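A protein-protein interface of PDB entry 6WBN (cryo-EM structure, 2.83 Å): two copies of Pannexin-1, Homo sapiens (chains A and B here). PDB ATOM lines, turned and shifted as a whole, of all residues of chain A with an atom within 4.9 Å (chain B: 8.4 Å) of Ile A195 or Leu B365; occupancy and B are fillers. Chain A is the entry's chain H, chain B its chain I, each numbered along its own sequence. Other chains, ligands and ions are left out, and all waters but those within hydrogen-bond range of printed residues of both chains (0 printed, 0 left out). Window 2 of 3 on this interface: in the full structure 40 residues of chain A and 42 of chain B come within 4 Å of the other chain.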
ATOM      1  N   PHE A 141      22.946  11.019   4.840  1.00  0.00           N
ATOM      2  CA  PHE A 141      22.281  12.314   4.787  1.00  0.00           C
ATOM      3  C   PHE A 141      22.399  13.051   6.112  1.00  0.00           C
ATOM      4  O   PHE A 141      22.609  14.271   6.137  1.00  0.00           O
ATOM      5  CB  PHE A 141      20.816  12.126   4.401  1.00  0.00           C
ATOM      6  CG  PHE A 141      19.932  13.247   4.844  1.00  0.00           C
ATOM      7  CD1 PHE A 141      19.761  14.369   4.055  1.00  0.00           C
ATOM      8  CD2 PHE A 141      19.267  13.177   6.058  1.00  0.00           C
ATOM      9  CE1 PHE A 141      18.947  15.399   4.470  1.00  0.00           C
ATOM     10  CE2 PHE A 141      18.462  14.204   6.476  1.00  0.00           C
ATOM     11  CZ  PHE A 141      18.299  15.315   5.683  1.00  0.00           C
ATOM     12  N   PRO A 194      17.395  23.354  11.688  1.00  0.00           N
ATOM     13  CA  PRO A 194      17.594  22.042  12.307  1.00  0.00           C
ATOM     14  C   PRO A 194      16.875  20.920  11.567  1.00  0.00           C
ATOM     15  O   PRO A 194      16.159  20.140  12.193  1.00  0.00           O
ATOM     16  CB  PRO A 194      16.994  22.219  13.701  1.00  0.00           C
ATOM     17  CG  PRO A 194      15.939  23.249  13.514  1.00  0.00           C
ATOM     18  CD  PRO A 194      16.450  24.187  12.452  1.00  0.00           C
ATOM     19  N   ILE A 195      17.074  20.825  10.251  1.00  0.00           N
ATOM     20  CA  ILE A 195      16.388  19.790   9.485  1.00  0.00           C
ATOM     21  C   ILE A 195      16.864  18.413   9.917  1.00  0.00           C
ATOM     22  O   ILE A 195      16.063  17.479  10.042  1.00  0.00           O
ATOM     23  CB  ILE A 195      16.590  20.011   7.976  1.00  0.00           C
ATOM     24  CG1 ILE A 195      16.182  21.431   7.576  1.00  0.00           C
ATOM     25  CG2 ILE A 195      15.784  19.001   7.180  1.00  0.00           C
ATOM     26  CD1 ILE A 195      14.927  21.944   8.274  1.00  0.00           C
ATOM     27  N   VAL A 196      18.163  18.268  10.177  1.00  0.00           N
ATOM     28  CA  VAL A 196      18.677  16.980  10.627  1.00  0.00           C
ATOM     29  C   VAL A 196      18.170  16.659  12.025  1.00  0.00           C
ATOM     30  O   VAL A 196      17.858  15.500  12.332  1.00  0.00           O
ATOM     31  CB  VAL A 196      20.214  16.965  10.546  1.00  0.00           C
ATOM     32  CG1 VAL A 196      20.831  17.994  11.478  1.00  0.00           C
ATOM     33  CG2 VAL A 196      20.751  15.577  10.851  1.00  0.00           C
ATOM     34  N   GLU A 197      18.036  17.670  12.881  1.00  0.00           N
ATOM     35  CA  GLU A 197      17.495  17.428  14.212  1.00  0.00           C
ATOM     36  C   GLU A 197      16.047  16.966  14.131  1.00  0.00           C
ATOM     37  O   GLU A 197      15.633  16.057  14.861  1.00  0.00           O
ATOM     38  CB  GLU A 197      17.610  18.691  15.061  1.00  0.00           C
ATOM     39  CG  GLU A 197      17.494  18.433  16.548  1.00  0.00           C
ATOM     40  CD  GLU A 197      16.067  18.493  17.039  1.00  0.00           C
ATOM     41  OE1 GLU A 197      15.257  19.211  16.418  1.00  0.00           O
ATOM     42  OE2 GLU A 197      15.755  17.813  18.038  1.00  0.00           O
ATOM     43  N   GLN A 198      15.264  17.568  13.238  1.00  0.00           N
ATOM     44  CA  GLN A 198      13.871  17.160  13.117  1.00  0.00           C
ATOM     45  C   GLN A 198      13.751  15.785  12.474  1.00  0.00           C
ATOM     46  O   GLN A 198      12.846  15.016  12.809  1.00  0.00           O
ATOM     47  CB  GLN A 198      13.082  18.206  12.339  1.00  0.00           C
ATOM     48  CG  GLN A 198      12.683  19.369  13.211  1.00  0.00           C
ATOM     49  CD  GLN A 198      11.969  18.909  14.461  1.00  0.00           C
ATOM     50  OE1 GLN A 198      12.328  19.299  15.570  1.00  0.00           O
ATOM     51  NE2 GLN A 198      10.955  18.070  14.289  1.00  0.00           N
ATOM     52  N   TYR A 199      14.658  15.450  11.554  1.00  0.00           N
ATOM     53  CA  TYR A 199      14.681  14.093  11.020  1.00  0.00           C
ATOM     54  C   TYR A 199      14.998  13.084  12.110  1.00  0.00           C
ATOM     55  O   TYR A 199      14.444  11.979  12.131  1.00  0.00           O
ATOM     56  CB  TYR A 199      15.699  13.979   9.892  1.00  0.00           C
ATOM     57  CG  TYR A 199      15.591  12.679   9.145  1.00  0.00           C
ATOM     58  CD1 TYR A 199      14.362  12.070   8.957  1.00  0.00           C
ATOM     59  CD2 TYR A 199      16.720  12.044   8.655  1.00  0.00           C
ATOM     60  CE1 TYR A 199      14.257  10.876   8.283  1.00  0.00           C
ATOM     61  CE2 TYR A 199      16.625  10.849   7.982  1.00  0.00           C
ATOM     62  CZ  TYR A 199      15.395  10.268   7.799  1.00  0.00           C
ATOM     63  OH  TYR A 199      15.303   9.074   7.125  1.00  0.00           O
ATOM     64  N   TYR B 150      12.011  18.316  -9.783  1.00  0.00           N
ATOM     65  CA  TYR B 150      12.295  18.816  -8.440  1.00  0.00           C
ATOM     66  C   TYR B 150      13.132  20.088  -8.494  1.00  0.00           C
ATOM     67  O   TYR B 150      12.934  21.013  -7.692  1.00  0.00           O
ATOM     68  CB  TYR B 150      13.003  17.744  -7.614  1.00  0.00           C
ATOM     69  CG  TYR B 150      13.554  18.250  -6.302  1.00  0.00           C
ATOM     70  CD1 TYR B 150      12.744  18.348  -5.180  1.00  0.00           C
ATOM     71  CD2 TYR B 150      14.887  18.622  -6.181  1.00  0.00           C
ATOM     72  CE1 TYR B 150      13.242  18.808  -3.976  1.00  0.00           C
ATOM     73  CE2 TYR B 150      15.394  19.083  -4.980  1.00  0.00           C
ATOM     74  CZ  TYR B 150      14.567  19.171  -3.881  1.00  0.00           C
ATOM     75  OH  TYR B 150      15.064  19.628  -2.684  1.00  0.00           O
ATOM     76  N   CYS B 347      16.172  13.851  -0.246  1.00  0.00           N
ATOM     77  CA  CYS B 347      15.824  15.127   0.367  1.00  0.00           C
ATOM     78  C   CYS B 347      14.320  15.278   0.509  1.00  0.00           C
ATOM     79  O   CYS B 347      13.819  15.703   1.559  1.00  0.00           O
ATOM     80  CB  CYS B 347      16.400  16.276  -0.451  1.00  0.00           C
ATOM     81  SG  CYS B 347      18.199  16.299  -0.463  1.00  0.00           S
ATOM     82  N   VAL B 350      12.989  13.060   3.394  1.00  0.00           N
ATOM     83  CA  VAL B 350      13.221  13.570   4.743  1.00  0.00           C
ATOM     84  C   VAL B 350      12.334  14.783   5.007  1.00  0.00           C
ATOM     85  O   VAL B 350      11.829  14.970   6.123  1.00  0.00           O
ATOM     86  CB  VAL B 350      14.713  13.870   4.979  1.00  0.00           C
ATOM     87  CG1 VAL B 350      15.279  14.719   3.892  1.00  0.00           C
ATOM     88  CG2 VAL B 350      14.925  14.519   6.329  1.00  0.00           C
ATOM     89  N   LEU B 351      12.098  15.611   3.981  1.00  0.00           N
ATOM     90  CA  LEU B 351      11.117  16.686   4.139  1.00  0.00           C
ATOM     91  C   LEU B 351       9.725  16.146   4.448  1.00  0.00           C
ATOM     92  O   LEU B 351       8.999  16.718   5.268  1.00  0.00           O
ATOM     93  CB  LEU B 351      11.071  17.573   2.896  1.00  0.00           C
ATOM     94  CG  LEU B 351      11.981  18.802   2.847  1.00  0.00           C
ATOM     95  CD1 LEU B 351      11.628  19.687   4.020  1.00  0.00           C
ATOM     96  CD2 LEU B 351      13.452  18.460   2.880  1.00  0.00           C
ATOM     97  N   GLU B 352       9.322  15.059   3.789  1.00  0.00           N
ATOM     98  CA  GLU B 352       8.011  14.479   4.073  1.00  0.00           C
ATOM     99  C   GLU B 352       7.949  13.924   5.489  1.00  0.00           C
ATOM    100  O   GLU B 352       6.910  13.993   6.153  1.00  0.00           O
ATOM    101  CB  GLU B 352       7.679  13.384   3.064  1.00  0.00           C
ATOM    102  CG  GLU B 352       6.195  13.056   3.000  1.00  0.00           C
ATOM    103  CD  GLU B 352       5.899  11.829   2.157  1.00  0.00           C
ATOM    104  OE1 GLU B 352       6.523  11.677   1.092  1.00  0.00           O
ATOM    105  OE2 GLU B 352       5.044  11.012   2.563  1.00  0.00           O
ATOM    106  N   ASN B 353       9.051  13.350   5.961  1.00  0.00           N
ATOM    107  CA  ASN B 353       9.097  12.874   7.338  1.00  0.00           C
ATOM    108  C   ASN B 353       8.978  14.031   8.321  1.00  0.00           C
ATOM    109  O   ASN B 353       8.304  13.917   9.348  1.00  0.00           O
ATOM    110  CB  ASN B 353      10.391  12.099   7.582  1.00  0.00           C
ATOM    111  CG  ASN B 353      10.211  10.603   7.448  1.00  0.00           C
ATOM    112  OD1 ASN B 353       9.247  10.126   6.845  1.00  0.00           O
ATOM    113  ND2 ASN B 353      11.144   9.851   8.015  1.00  0.00           N
ATOM    114  N   ILE B 354       9.645  15.148   8.032  1.00  0.00           N
ATOM    115  CA  ILE B 354       9.505  16.332   8.877  1.00  0.00           C
ATOM    116  C   ILE B 354       8.064  16.818   8.847  1.00  0.00           C
ATOM    117  O   ILE B 354       7.522  17.279   9.861  1.00  0.00           O
ATOM    118  CB  ILE B 354      10.482  17.437   8.434  1.00  0.00           C
ATOM    119  CG1 ILE B 354      11.913  16.917   8.467  1.00  0.00           C
ATOM    120  CG2 ILE B 354      10.370  18.643   9.347  1.00  0.00           C
ATOM    121  CD1 ILE B 354      12.283  16.291   9.770  1.00  0.00           C
ATOM    122  N   LYS B 355       7.424  16.731   7.680  1.00  0.00           N
ATOM    123  CA  LYS B 355       5.999  17.025   7.595  1.00  0.00           C
ATOM    124  C   LYS B 355       5.205  16.106   8.509  1.00  0.00           C
ATOM    125  O   LYS B 355       4.244  16.536   9.158  1.00  0.00           O
ATOM    126  CB  LYS B 355       5.520  16.892   6.151  1.00  0.00           C
ATOM    127  CG  LYS B 355       4.042  17.232   5.903  1.00  0.00           C
ATOM    128  CD  LYS B 355       3.523  18.480   6.637  1.00  0.00           C
ATOM    129  CE  LYS B 355       4.363  19.733   6.391  1.00  0.00           C
ATOM    130  NZ  LYS B 355       3.551  20.979   6.512  1.00  0.00           N
ATOM    131  N   GLN B 359       6.709  20.327  11.969  1.00  0.00           N
ATOM    132  CA  GLN B 359       7.304  21.437  12.704  1.00  0.00           C
ATOM    133  C   GLN B 359       7.397  22.705  11.860  1.00  0.00           C
ATOM    134  O   GLN B 359       6.867  23.752  12.246  1.00  0.00           O
ATOM    135  CB  GLN B 359       8.691  21.036  13.224  1.00  0.00           C
ATOM    136  N   GLY B 360       8.066  22.632  10.711  1.00  0.00           N
ATOM    137  CA  GLY B 360       8.260  23.806   9.882  1.00  0.00           C
ATOM    138  C   GLY B 360       7.365  23.876   8.662  1.00  0.00           C
ATOM    139  O   GLY B 360       6.136  23.866   8.775  1.00  0.00           O
ATOM    140  N   ILE B 361       7.980  23.955   7.485  1.00  0.00           N
ATOM    141  CA  ILE B 361       7.253  24.040   6.224  1.00  0.00           C
ATOM    142  C   ILE B 361       8.113  23.417   5.138  1.00  0.00           C
ATOM    143  O   ILE B 361       9.340  23.343   5.256  1.00  0.00           O
ATOM    144  CB  ILE B 361       6.884  25.498   5.866  1.00  0.00           C
ATOM    145  N   ASP B 362       7.455  22.961   4.068  1.00  0.00           N
ATOM    146  CA  ASP B 362       8.184  22.291   2.993  1.00  0.00           C
ATOM    147  C   ASP B 362       9.117  23.236   2.240  1.00  0.00           C
ATOM    148  O   ASP B 362      10.324  22.946   2.169  1.00  0.00           O
ATOM    149  CB  ASP B 362       7.198  21.593   2.053  1.00  0.00           C
ATOM    150  N   PRO B 363       8.656  24.358   1.670  1.00  0.00           N
ATOM    151  CA  PRO B 363       9.564  25.132   0.807  1.00  0.00           C
ATOM    152  C   PRO B 363      10.719  25.768   1.559  1.00  0.00           C
ATOM    153  O   PRO B 363      11.833  25.835   1.025  1.00  0.00           O
ATOM    154  CB  PRO B 363       8.640  26.188   0.190  1.00  0.00           C
ATOM    155  CG  PRO B 363       7.577  26.374   1.205  1.00  0.00           C
ATOM    156  CD  PRO B 363       7.339  25.011   1.788  1.00  0.00           C
ATOM    157  N   MET B 364      10.488  26.235   2.787  1.00  0.00           N
ATOM    158  CA  MET B 364      11.554  26.891   3.539  1.00  0.00           C
ATOM    159  C   MET B 364      12.693  25.922   3.832  1.00  0.00           C
ATOM    160  O   MET B 364      13.863  26.213   3.552  1.00  0.00           O
ATOM    161  CB  MET B 364      10.994  27.474   4.836  1.00  0.00           C
ATOM    162  N   LEU B 365      12.364  24.755   4.387  1.00  0.00           N
ATOM    163  CA  LEU B 365      13.393  23.767   4.685  1.00  0.00           C
ATOM    164  C   LEU B 365      14.005  23.189   3.416  1.00  0.00           C
ATOM    165  O   LEU B 365      15.166  22.769   3.428  1.00  0.00           O
ATOM    166  CB  LEU B 365      12.814  22.656   5.559  1.00  0.00           C
ATOM    167  N   LEU B 366      13.246  23.147   2.319  1.00  0.00           N
ATOM    168  CA  LEU B 366      13.817  22.699   1.052  1.00  0.00           C
ATOM    169  C   LEU B 366      14.872  23.680   0.555  1.00  0.00           C
ATOM    170  O   LEU B 366      15.946  23.274   0.094  1.00  0.00           O
ATOM    171  CB  LEU B 366      12.713  22.518   0.009  1.00  0.00           C
ATOM    172  N   LEU B 367      14.576  24.979   0.628  1.00  0.00           N
ATOM    173  CA  LEU B 367      15.566  25.987   0.265  1.00  0.00           C
ATOM    174  C   LEU B 367      16.765  25.937   1.206  1.00  0.00           C
ATOM    175  O   LEU B 367      17.904  26.180   0.789  1.00  0.00           O
ATOM    176  CB  LEU B 367      14.931  27.376   0.277  1.00  0.00           C
ATOM    177  N   THR B 368      16.525  25.630   2.483  1.00  0.00           N
ATOM    178  CA  THR B 368      17.628  25.495   3.430  1.00  0.00           C
ATOM    179  C   THR B 368      18.510  24.296   3.093  1.00  0.00           C
ATOM    180  O   THR B 368      19.732  24.349   3.266  1.00  0.00           O
ATOM    181  CB  THR B 368      17.088  25.375   4.855  1.00  0.00           C
ATOM    182  N   ASN B 369      17.901  23.196   2.637  1.00  0.00           N
ATOM    183  CA  ASN B 369      18.610  21.967   2.283  1.00  0.00           C
ATOM    184  C   ASN B 369      19.827  22.231   1.403  1.00  0.00           C
ATOM    185  O   ASN B 369      20.951  21.876   1.776  1.00  0.00           O
ATOM    186  CB  ASN B 369      17.665  20.991   1.579  1.00  0.00           C
ATOM    187  N   LEU B 370      19.610  22.844   0.237  1.00  0.00           N
ATOM    188  CA  LEU B 370      20.675  23.143  -0.721  1.00  0.00           C
ATOM    189  C   LEU B 370      21.350  21.854  -1.197  1.00  0.00           C
ATOM    190  O   LEU B 370      22.551  21.632  -1.016  1.00  0.00           O
ATOM    191  CB  LEU B 370      21.689  24.127  -0.125  1.00  0.00           C
ATOM    192  N   GLY B 371      20.537  21.001  -1.813  1.00  0.00           N
ATOM    193  CA  GLY B 371      20.951  19.703  -2.312  1.00  0.00           C
ATOM    194  C   GLY B 371      20.678  19.515  -3.793  1.00  0.00           C
ATOM    195  O   GLY B 371      20.220  18.445  -4.211  1.00  0.00           O
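OE1 of Glu A197 sits close to OE1 of Gln A198 (3.1 Å).
CG2 of Val B350 touches CZ of Phe A141 (3.5 Å). CD1 of Ile B354 touches O of Ile A195 (3.97 Å). Leu B365 touches Ile A195 (CB to CD1, 3.5 Å). CD1 of Ile B354 touches C of Gln A198 (3.1 Å). Gln A198 touches Gln B359 (NE2 to CB, 3.9 Å). CG2 of Val B350 touches CG of Tyr A199 (3.4 Å). Asn B353 touches Tyr A199 (ND2 to CE1, 3.3 Å). N of Tyr A199 touches CD1 of Ile B354, at 3.1 Å.
Leu B365 touches one residue of chain A. No residue of chain B comes within 4 Å of Pro A194. Of the printed residues of chain A, Asn B353 touches Tyr A199 (3.3 Å). Of the printed residues of chain B, Gln A198 touches Ile B354 and Gln B359. Of the printed residues of chain A, Gln B359 touches Gln A198 (3.9 Å). Printed residues of chain B within 4 Å of Phe A141: Val B350 (3.5 Å). Pro B363 touches none of the printed residues of chain A. Leu B367 touches none of the printed residues of chain A. The nearest residue of chain B that does not touch Ile A195 is Val B350 (4.6 Å). The nearest printed residue of chain A that does not touch Leu B365 is Pro A194 (7.5 Å). The nearest printed residue of chain A that does not touch Asn B353 is Gln A198 (5.8 Å).
Hydrophobic or aromatic side chains of chain B that line the printed part of chain A: Val B350, Ile B354 and Leu B365. Of the 7 printed residues of chain A, 4 touch a printed residue of chain B. Among the printed residues, no Asp or Glu carboxylate lies within 4 Å of a Lys or Arg side-chain nitrogen of the other chain.
No position is printed for both chains. Of the 8 pairs that touch across the chains among the printed residues, none has its exchanged pair printed and touching as well.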
